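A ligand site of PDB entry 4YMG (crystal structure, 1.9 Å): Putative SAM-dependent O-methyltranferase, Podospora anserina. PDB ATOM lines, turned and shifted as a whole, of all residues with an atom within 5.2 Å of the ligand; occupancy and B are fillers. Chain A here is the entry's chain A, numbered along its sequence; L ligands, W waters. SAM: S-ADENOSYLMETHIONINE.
The side-chain carboxylate (OE2) of Glu 98 lies within hydrogen-bond range of the backbone NH (N) of Ser 100, at 3.0 Å.
The side-chain carboxylate (OE1) of Glu 98 lies within hydrogen-bond range of the backbone NH (N) of Tyr 75, at 2.7 Å.
The backbone carbonyl oxygen of Ile 72 is in hydrogen-bond range of the backbone NH of Ala 145 (3.2 Å).
OH of Tyr 153 lies within hydrogen-bond range of OD1 of Asn 146, at 2.5 Å.
OG of Ser 100 sits at hydrogen-bond distance from N of Met 103, at 3.2 Å.
N of Cys 74 is in hydrogen-bond range of O of Leu 97, 3.1 Å away.
The side-chain carboxylate (OE1) of Glu 98 is in hydrogen-bond range of the backbone NH (N) of Cys 74, at 3.2 Å.
The backbone NH (N) of Gly 73 lies within hydrogen-bond range of the backbone carbonyl oxygen (O) of Leu 97, 2.8 Å away.
Water W1 lies within hydrogen-bond range of O of the ligand (2.7 Å), N of Tyr 78 (3.0 Å) and O of Cys 74 (3.4 Å).
Water W3 lies within hydrogen-bond range of NZ of Lys 47 (2.9 Å) and O2' of the ligand (3.0 Å).
The backbone NH (N) of Tyr 99 sits close to a nitrogen (N3) of the ligand (3.4 Å).
N of the ligand is in hydrogen-bond range of OG of Ser 79 (2.7 Å).
The side-chain hydroxyl of Ser 49 sits at hydrogen-bond distance from an oxygen (OXT) of the ligand (2.5 Å).
A nitrogen (N6) of the ligand lies within hydrogen-bond range of the side-chain carboxylate (OE1) of Glu 128, at 3.0 Å.
The backbone NH (N) of Tyr 75 lies close to an oxygen (O3') of the ligand (3.3 Å).
The backbone NH (N) of Ala 127 is in hydrogen-bond range of a nitrogen (N1) of the ligand.
An oxygen (O2') of the ligand lies within hydrogen-bond range of the side-chain carboxylate of Glu 98, at 2.5 Å.
The side-chain hydroxyl of Tyr 153 lies within hydrogen-bond range of a nitrogen (N6) of the ligand, 3.2 Å away.
O of Gly 73 sits at hydrogen-bond distance from N of the ligand (2.8 Å).
The side-chain carboxylate of Asp 144 lies within salt-bridge range of a nitrogen (N) of the ligand (2.7 Å).
The side-chain amide oxygen (OD1) of Asn 146 is in hydrogen-bond range of a nitrogen (N6) of the ligand (3.2 Å).
O of the ligand is in hydrogen-bond range of N of Ser 49 (3.2 Å).
O of Lys 47 sits close to SD of the ligand (3.7 Å).
Residues that only touch the ligand: Met 48 (3.4 Å), Cys 74 (3.8 Å), Tyr 78 (3.5 Å), Ser 100 (3.8 Å), Gly 125 (3.7 Å), Pro 126 (3.6 Å) and Ala 145 (3.5 Å).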
ATOM      1  N   LYS A  47     -14.787  20.013 -28.983  1.00  0.00           N
ATOM      2  CA  LYS A  47     -14.302  18.640 -28.848  1.00  0.00           C
ATOM      3  C   LYS A  47     -15.362  17.626 -29.269  1.00  0.00           C
ATOM      4  O   LYS A  47     -15.043  16.500 -29.656  1.00  0.00           O
ATOM      5  CB  LYS A  47     -13.863  18.361 -27.413  1.00  0.00           C
ATOM      6  CG  LYS A  47     -12.664  19.173 -26.963  1.00  0.00           C
ATOM      7  CD  LYS A  47     -12.047  18.557 -25.694  1.00  0.00           C
ATOM      8  CE  LYS A  47     -10.767  19.273 -25.283  1.00  0.00           C
ATOM      9  NZ  LYS A  47      -9.986  18.501 -24.255  1.00  0.00           N
ATOM     10  N   MET A  48     -16.631  18.006 -29.173  1.00  0.00           N
ATOM     11  CA  MET A  48     -17.734  17.081 -29.442  1.00  0.00           C
ATOM     12  C   MET A  48     -17.933  16.821 -30.942  1.00  0.00           C
ATOM     13  O   MET A  48     -17.800  17.731 -31.759  1.00  0.00           O
ATOM     14  CB  MET A  48     -19.022  17.631 -28.842  1.00  0.00           C
ATOM     15  CG  MET A  48     -20.222  16.706 -29.017  1.00  0.00           C
ATOM     16  SD  MET A  48     -21.651  17.319 -28.103  1.00  0.00           S
ATOM     17  CE  MET A  48     -21.788  18.985 -28.762  1.00  0.00           C
ATOM     18  N   SER A  49     -18.244  15.585 -31.302  1.00  0.00           N
ATOM     19  CA  SER A  49     -18.541  15.232 -32.697  1.00  0.00           C
ATOM     20  C   SER A  49     -19.723  16.044 -33.210  1.00  0.00           C
ATOM     21  O   SER A  49     -20.515  16.576 -32.421  1.00  0.00           O
ATOM     22  CB  SER A  49     -18.851  13.725 -32.826  1.00  0.00           C
ATOM     23  OG  SER A  49     -17.718  12.958 -32.469  1.00  0.00           O
ATOM     24  N   MET A  57     -22.515   7.523 -36.702  1.00  0.00           N
ATOM     25  CA  MET A  57     -22.286   6.567 -35.638  1.00  0.00           C
ATOM     26  C   MET A  57     -23.499   5.656 -35.437  1.00  0.00           C
ATOM     27  O   MET A  57     -23.369   4.436 -35.369  1.00  0.00           O
ATOM     28  CB  MET A  57     -21.940   7.277 -34.339  1.00  0.00           C
ATOM     29  CG  MET A  57     -20.624   8.032 -34.411  1.00  0.00           C
ATOM     30  SD  MET A  57     -20.311   8.948 -32.884  1.00  0.00           S
ATOM     31  CE  MET A  57     -21.619  10.095 -32.850  1.00  0.00           C
ATOM     32  N   GLU A  71     -15.192   2.915 -26.561  1.00  0.00           N
ATOM     33  CA  GLU A  71     -14.720   4.174 -27.093  1.00  0.00           C
ATOM     34  C   GLU A  71     -13.738   4.799 -26.114  1.00  0.00           C
ATOM     35  O   GLU A  71     -13.835   4.618 -24.887  1.00  0.00           O
ATOM     36  CB  GLU A  71     -15.883   5.130 -27.424  1.00  0.00           C
ATOM     37  CG  GLU A  71     -16.568   5.737 -26.252  1.00  0.00           C
ATOM     38  CD  GLU A  71     -17.516   6.861 -26.666  1.00  0.00           C
ATOM     39  OE1 GLU A  71     -17.882   6.962 -27.862  1.00  0.00           O
ATOM     40  OE2 GLU A  71     -17.878   7.655 -25.777  1.00  0.00           O
ATOM     41  N   ILE A  72     -12.763   5.494 -26.674  1.00  0.00           N
ATOM     42  CA  ILE A  72     -11.778   6.203 -25.870  1.00  0.00           C
ATOM     43  C   ILE A  72     -11.967   7.709 -26.048  1.00  0.00           C
ATOM     44  O   ILE A  72     -11.766   8.241 -27.144  1.00  0.00           O
ATOM     45  CB  ILE A  72     -10.352   5.785 -26.235  1.00  0.00           C
ATOM     46  CG1 ILE A  72     -10.253   4.255 -26.288  1.00  0.00           C
ATOM     47  CG2 ILE A  72      -9.355   6.397 -25.233  1.00  0.00           C
ATOM     48  CD1 ILE A  72      -8.887   3.732 -26.678  1.00  0.00           C
ATOM     49  N   GLY A  73     -12.376   8.388 -24.977  1.00  0.00           N
ATOM     50  CA  GLY A  73     -12.664   9.814 -25.043  1.00  0.00           C
ATOM     51  C   GLY A  73     -14.157  10.087 -24.993  1.00  0.00           C
ATOM     52  O   GLY A  73     -14.809  10.321 -26.015  1.00  0.00           O
ATOM     53  N   CYS A  74     -14.712  10.067 -23.794  1.00  0.00           N
ATOM     54  CA  CYS A  74     -16.145  10.238 -23.616  1.00  0.00           C
ATOM     55  C   CYS A  74     -16.580  11.690 -23.822  1.00  0.00           C
ATOM     56  O   CYS A  74     -17.645  11.958 -24.388  1.00  0.00           O
ATOM     57  CB  CYS A  74     -16.562   9.779 -22.229  1.00  0.00           C
ATOM     58  SG  CYS A  74     -18.350   9.655 -22.051  1.00  0.00           S
ATOM     59  N   TYR A  75     -15.752  12.613 -23.336  1.00  0.00           N
ATOM     60  CA  TYR A  75     -16.121  14.028 -23.235  1.00  0.00           C
ATOM     61  C   TYR A  75     -17.478  14.181 -22.508  1.00  0.00           C
ATOM     62  O   TYR A  75     -17.553  13.891 -21.316  1.00  0.00           O
ATOM     63  CB  TYR A  75     -16.129  14.695 -24.620  1.00  0.00           C
ATOM     64  CG  TYR A  75     -16.282  16.197 -24.540  1.00  0.00           C
ATOM     65  CD1 TYR A  75     -15.351  16.986 -23.837  1.00  0.00           C
ATOM     66  CD2 TYR A  75     -17.351  16.845 -25.147  1.00  0.00           C
ATOM     67  CE1 TYR A  75     -15.495  18.354 -23.756  1.00  0.00           C
ATOM     68  CE2 TYR A  75     -17.505  18.211 -25.065  1.00  0.00           C
ATOM     69  CZ  TYR A  75     -16.585  18.955 -24.362  1.00  0.00           C
ATOM     70  OH  TYR A  75     -16.758  20.316 -24.279  1.00  0.00           O
ATOM     71  N   TYR A  78     -21.633  12.335 -25.819  1.00  0.00           N
ATOM     72  CA  TYR A  78     -22.358  12.378 -27.083  1.00  0.00           C
ATOM     73  C   TYR A  78     -22.215  11.102 -27.917  1.00  0.00           C
ATOM     74  O   TYR A  78     -23.214  10.506 -28.327  1.00  0.00           O
ATOM     75  CB  TYR A  78     -21.911  13.581 -27.909  1.00  0.00           C
ATOM     76  CG  TYR A  78     -22.552  13.683 -29.270  1.00  0.00           C
ATOM     77  CD1 TYR A  78     -23.920  13.943 -29.402  1.00  0.00           C
ATOM     78  CD2 TYR A  78     -21.797  13.548 -30.432  1.00  0.00           C
ATOM     79  CE1 TYR A  78     -24.515  14.051 -30.651  1.00  0.00           C
ATOM     80  CE2 TYR A  78     -22.395  13.663 -31.694  1.00  0.00           C
ATOM     81  CZ  TYR A  78     -23.744  13.894 -31.788  1.00  0.00           C
ATOM     82  OH  TYR A  78     -24.322  14.016 -33.040  1.00  0.00           O
ATOM     83  N   SER A  79     -20.969  10.690 -28.170  1.00  0.00           N
ATOM     84  CA  SER A  79     -20.754   9.548 -29.047  1.00  0.00           C
ATOM     85  C   SER A  79     -21.191   8.271 -28.316  1.00  0.00           C
ATOM     86  O   SER A  79     -21.732   7.361 -28.939  1.00  0.00           O
ATOM     87  CB  SER A  79     -19.292   9.452 -29.510  1.00  0.00           C
ATOM     88  OG  SER A  79     -18.361   9.587 -28.454  1.00  0.00           O
ATOM     89  N   LEU A  97     -14.071   5.464 -22.066  1.00  0.00           N
ATOM     90  CA  LEU A  97     -12.946   5.914 -21.251  1.00  0.00           C
ATOM     91  C   LEU A  97     -12.810   7.441 -21.219  1.00  0.00           C
ATOM     92  O   LEU A  97     -12.888   8.090 -22.260  1.00  0.00           O
ATOM     93  CB  LEU A  97     -11.647   5.295 -21.752  1.00  0.00           C
ATOM     94  CG  LEU A  97     -11.639   3.777 -21.931  1.00  0.00           C
ATOM     95  CD1 LEU A  97     -10.249   3.291 -22.279  1.00  0.00           C
ATOM     96  CD2 LEU A  97     -12.118   3.105 -20.667  1.00  0.00           C
ATOM     97  N   GLU A  98     -12.591   7.999 -20.037  1.00  0.00           N
ATOM     98  CA  GLU A  98     -12.449   9.443 -19.872  1.00  0.00           C
ATOM     99  C   GLU A  98     -11.593   9.733 -18.627  1.00  0.00           C
ATOM    100  O   GLU A  98     -11.699   9.020 -17.631  1.00  0.00           O
ATOM    101  CB  GLU A  98     -13.848  10.092 -19.758  1.00  0.00           C
ATOM    102  CG  GLU A  98     -13.839  11.603 -19.496  1.00  0.00           C
ATOM    103  CD  GLU A  98     -13.146  12.367 -20.587  1.00  0.00           C
ATOM    104  OE1 GLU A  98     -13.541  12.191 -21.768  1.00  0.00           O
ATOM    105  OE2 GLU A  98     -12.199  13.130 -20.269  1.00  0.00           O
ATOM    106  N   TYR A  99     -10.772  10.732 -18.695  1.00  0.00           N
ATOM    107  CA  TYR A  99      -9.924  11.071 -17.585  1.00  0.00           C
ATOM    108  C   TYR A  99     -10.211  12.397 -16.927  1.00  0.00           C
ATOM    109  O   TYR A  99      -9.729  12.657 -15.880  1.00  0.00           O
ATOM    110  CB  TYR A  99      -8.455  10.963 -17.973  1.00  0.00           C
ATOM    111  CG  TYR A  99      -7.839  12.121 -18.717  1.00  0.00           C
ATOM    112  CD1 TYR A  99      -6.510  12.359 -18.582  1.00  0.00           C
ATOM    113  CD2 TYR A  99      -8.552  12.945 -19.593  1.00  0.00           C
ATOM    114  CE1 TYR A  99      -5.878  13.365 -19.268  1.00  0.00           C
ATOM    115  CE2 TYR A  99      -7.919  13.993 -20.280  1.00  0.00           C
ATOM    116  CZ  TYR A  99      -6.578  14.189 -20.114  1.00  0.00           C
ATOM    117  OH  TYR A  99      -5.893  15.199 -20.750  1.00  0.00           O
ATOM    118  N   SER A 100     -10.948  13.250 -17.574  1.00  0.00           N
ATOM    119  CA  SER A 100     -11.255  14.552 -16.993  1.00  0.00           C
ATOM    120  C   SER A 100     -12.309  14.443 -15.895  1.00  0.00           C
ATOM    121  O   SER A 100     -13.401  13.941 -16.131  1.00  0.00           O
ATOM    122  CB  SER A 100     -11.724  15.525 -18.060  1.00  0.00           C
ATOM    123  OG  SER A 100     -12.392  16.611 -17.457  1.00  0.00           O
ATOM    124  N   MET A 103     -15.560  16.266 -16.946  1.00  0.00           N
ATOM    125  CA  MET A 103     -16.351  15.638 -17.996  1.00  0.00           C
ATOM    126  C   MET A 103     -16.885  14.269 -17.551  1.00  0.00           C
ATOM    127  O   MET A 103     -17.919  13.810 -18.056  1.00  0.00           O
ATOM    128  CB  MET A 103     -15.532  15.511 -19.273  1.00  0.00           C
ATOM    129  CG  MET A 103     -15.051  16.864 -19.817  1.00  0.00           C
ATOM    130  SD  MET A 103     -16.317  18.150 -19.775  1.00  0.00           S
ATOM    131  CE  MET A 103     -17.501  17.504 -20.954  1.00  0.00           C
ATOM    132  N   GLY A 125     -10.288   7.597 -15.624  1.00  0.00           N
ATOM    133  CA  GLY A 125      -8.843   7.581 -15.520  1.00  0.00           C
ATOM    134  C   GLY A 125      -8.130   7.735 -16.845  1.00  0.00           C
ATOM    135  O   GLY A 125      -8.759   7.671 -17.898  1.00  0.00           O
ATOM    136  N   PRO A 126      -6.813   7.957 -16.808  1.00  0.00           N
ATOM    137  CA  PRO A 126      -6.063   8.054 -18.057  1.00  0.00           C
ATOM    138  C   PRO A 126      -6.175   6.741 -18.841  1.00  0.00           C
ATOM    139  O   PRO A 126      -6.000   5.676 -18.265  1.00  0.00           O
ATOM    140  CB  PRO A 126      -4.630   8.320 -17.600  1.00  0.00           C
ATOM    141  CG  PRO A 126      -4.766   8.866 -16.209  1.00  0.00           C
ATOM    142  CD  PRO A 126      -5.951   8.160 -15.624  1.00  0.00           C
ATOM    143  N   ALA A 127      -6.511   6.830 -20.117  1.00  0.00           N
ATOM    144  CA  ALA A 127      -6.754   5.638 -20.929  1.00  0.00           C
ATOM    145  C   ALA A 127      -5.505   4.773 -21.093  1.00  0.00           C
ATOM    146  O   ALA A 127      -5.610   3.578 -21.267  1.00  0.00           O
ATOM    147  CB  ALA A 127      -7.288   6.037 -22.300  1.00  0.00           C
ATOM    148  N   GLU A 128      -4.326   5.387 -21.048  1.00  0.00           N
ATOM    149  CA  GLU A 128      -3.085   4.628 -21.114  1.00  0.00           C
ATOM    150  C   GLU A 128      -3.082   3.538 -20.038  1.00  0.00           C
ATOM    151  O   GLU A 128      -2.614   2.430 -20.276  1.00  0.00           O
ATOM    152  CB  GLU A 128      -1.863   5.536 -20.986  1.00  0.00           C
ATOM    153  CG  GLU A 128      -1.968   6.605 -19.907  1.00  0.00           C
ATOM    154  CD  GLU A 128      -2.458   7.943 -20.445  1.00  0.00           C
ATOM    155  OE1 GLU A 128      -3.348   7.944 -21.328  1.00  0.00           O
ATOM    156  OE2 GLU A 128      -1.947   8.996 -19.990  1.00  0.00           O
ATOM    157  N   PHE A 142     -13.887   2.864 -30.975  1.00  0.00           N
ATOM    158  CA  PHE A 142     -13.888   4.235 -31.460  1.00  0.00           C
ATOM    159  C   PHE A 142     -12.831   5.025 -30.697  1.00  0.00           C
ATOM    160  O   PHE A 142     -12.970   5.260 -29.498  1.00  0.00           O
ATOM    161  CB  PHE A 142     -15.261   4.871 -31.292  1.00  0.00           C
ATOM    162  CG  PHE A 142     -15.360   6.300 -31.833  1.00  0.00           C
ATOM    163  CD1 PHE A 142     -14.996   6.598 -33.140  1.00  0.00           C
ATOM    164  CD2 PHE A 142     -15.882   7.329 -31.041  1.00  0.00           C
ATOM    165  CE1 PHE A 142     -15.117   7.905 -33.640  1.00  0.00           C
ATOM    166  CE2 PHE A 142     -16.004   8.636 -31.542  1.00  0.00           C
ATOM    167  CZ  PHE A 142     -15.625   8.917 -32.845  1.00  0.00           C
ATOM    168  N   ASP A 144     -10.959   8.338 -29.978  1.00  0.00           N
ATOM    169  CA  ASP A 144     -11.308   9.743 -30.111  1.00  0.00           C
ATOM    170  C   ASP A 144     -10.805  10.550 -28.917  1.00  0.00           C
ATOM    171  O   ASP A 144     -11.477  11.440 -28.421  1.00  0.00           O
ATOM    172  CB  ASP A 144     -12.835   9.888 -30.256  1.00  0.00           C
ATOM    173  CG  ASP A 144     -13.259  11.279 -30.683  1.00  0.00           C
ATOM    174  OD1 ASP A 144     -12.478  11.983 -31.369  1.00  0.00           O
ATOM    175  OD2 ASP A 144     -14.392  11.666 -30.342  1.00  0.00           O
ATOM    176  N   ALA A 145      -9.612  10.239 -28.433  1.00  0.00           N
ATOM    177  CA  ALA A 145      -9.102  10.998 -27.311  1.00  0.00           C
ATOM    178  C   ALA A 145      -7.815  11.712 -27.702  1.00  0.00           C
ATOM    179  O   ALA A 145      -7.776  12.391 -28.730  1.00  0.00           O
ATOM    180  CB  ALA A 145      -8.887  10.097 -26.096  1.00  0.00           C
ATOM    181  N   ASN A 146      -6.779  11.591 -26.893  1.00  0.00           N
ATOM    182  CA  ASN A 146      -5.581  12.367 -27.155  1.00  0.00           C
ATOM    183  C   ASN A 146      -4.824  11.841 -28.367  1.00  0.00           C
ATOM    184  O   ASN A 146      -4.436  10.673 -28.425  1.00  0.00           O
ATOM    185  CB  ASN A 146      -4.664  12.425 -25.926  1.00  0.00           C
ATOM    186  CG  ASN A 146      -4.267  11.075 -25.436  1.00  0.00           C
ATOM    187  OD1 ASN A 146      -5.122  10.234 -25.159  1.00  0.00           O
ATOM    188  ND2 ASN A 146      -2.957  10.844 -25.301  1.00  0.00           N
ATOM    189  N   TYR A 153      -2.583   3.375 -27.983  1.00  0.00           N
ATOM    190  CA  TYR A 153      -3.918   2.769 -27.844  1.00  0.00           C
ATOM    191  C   TYR A 153      -4.095   1.576 -28.770  1.00  0.00           C
ATOM    192  O   TYR A 153      -4.469   0.497 -28.334  1.00  0.00           O
ATOM    193  CB  TYR A 153      -5.022   3.799 -28.101  1.00  0.00           C
ATOM    194  CG  TYR A 153      -5.057   4.914 -27.074  1.00  0.00           C
ATOM    195  CD1 TYR A 153      -4.607   4.688 -25.776  1.00  0.00           C
ATOM    196  CD2 TYR A 153      -5.520   6.185 -27.390  1.00  0.00           C
ATOM    197  CE1 TYR A 153      -4.621   5.683 -24.833  1.00  0.00           C
ATOM    198  CE2 TYR A 153      -5.538   7.203 -26.433  1.00  0.00           C
ATOM    199  CZ  TYR A 153      -5.079   6.935 -25.145  1.00  0.00           C
ATOM    200  OH  TYR A 153      -5.065   7.903 -24.164  1.00  0.00           O
ATOM    201  N   ASN A 173     -10.550  12.047 -36.306  1.00  0.00           N
ATOM    202  CA  ASN A 173      -9.736  13.265 -36.375  1.00  0.00           C
ATOM    203  C   ASN A 173      -8.269  13.025 -36.783  1.00  0.00           C
ATOM    204  O   ASN A 173      -7.380  13.746 -36.362  1.00  0.00           O
ATOM    205  CB  ASN A 173      -9.753  14.009 -35.022  1.00  0.00           C
ATOM    206  CG  ASN A 173     -11.152  14.457 -34.603  1.00  0.00           C
ATOM    207  OD1 ASN A 173     -11.806  13.817 -33.778  1.00  0.00           O
ATOM    208  ND2 ASN A 173     -11.605  15.576 -35.170  1.00  0.00           N
HETATM  209  N   SAM L   1     -16.086  11.100 -28.371  1.00  0.00           N
HETATM  210  CA  SAM L   1     -16.613  12.414 -28.009  1.00  0.00           C
HETATM  211  C   SAM L   1     -17.699  12.867 -28.970  1.00  0.00           C
HETATM  212  O   SAM L   1     -18.460  13.786 -28.665  1.00  0.00           O
HETATM  213  OXT SAM L   1     -17.836  12.329 -30.064  1.00  0.00           O
HETATM  214  CB  SAM L   1     -15.537  13.507 -27.935  1.00  0.00           C
HETATM  215  CG  SAM L   1     -14.165  13.087 -27.425  1.00  0.00           C
HETATM  216  SD  SAM L   1     -13.107  14.542 -27.140  1.00  0.00           S
HETATM  217  CE  SAM L   1     -12.445  14.745 -28.826  1.00  0.00           C
HETATM  218  C5' SAM L   1     -11.644  13.834 -26.335  1.00  0.00           C
HETATM  219  C4' SAM L   1     -11.876  13.387 -24.899  1.00  0.00           C
HETATM  220  O4' SAM L   1     -10.816  12.542 -24.491  1.00  0.00           O
HETATM  221  C3' SAM L   1     -11.894  14.551 -23.905  1.00  0.00           C
HETATM  222  O3' SAM L   1     -13.036  14.447 -23.095  1.00  0.00           O
HETATM  223  C2' SAM L   1     -10.656  14.364 -23.039  1.00  0.00           C
HETATM  224  O2' SAM L   1     -10.835  14.723 -21.685  1.00  0.00           O
HETATM  225  C1' SAM L   1     -10.417  12.879 -23.174  1.00  0.00           C
HETATM  226  N9  SAM L   1      -9.006  12.517 -23.028  1.00  0.00           N
HETATM  227  C8  SAM L   1      -7.904  13.159 -23.535  1.00  0.00           C
HETATM  228  N7  SAM L   1      -6.807  12.457 -23.183  1.00  0.00           N
HETATM  229  C5  SAM L   1      -7.205  11.376 -22.468  1.00  0.00           C
HETATM  230  C6  SAM L   1      -6.510  10.330 -21.877  1.00  0.00           C
HETATM  231  N6  SAM L   1      -5.175  10.260 -21.935  1.00  0.00           N
HETATM  232  N1  SAM L   1      -7.232   9.352 -21.208  1.00  0.00           N
HETATM  233  C2  SAM L   1      -8.601   9.397 -21.134  1.00  0.00           C
HETATM  234  N3  SAM L   1      -9.284  10.435 -21.722  1.00  0.00           N
HETATM  235  C4  SAM L   1      -8.590  11.400 -22.378  1.00  0.00           C
HETATM  236  O   HOH W   1     -19.391  14.267 -26.156  1.00  0.00           O
HETATM  237  O   HOH W   2      -3.893  12.898 -22.523  1.00  0.00           O
HETATM  238  O   HOH W   3     -11.769  17.527 -22.185  1.00  0.00           O
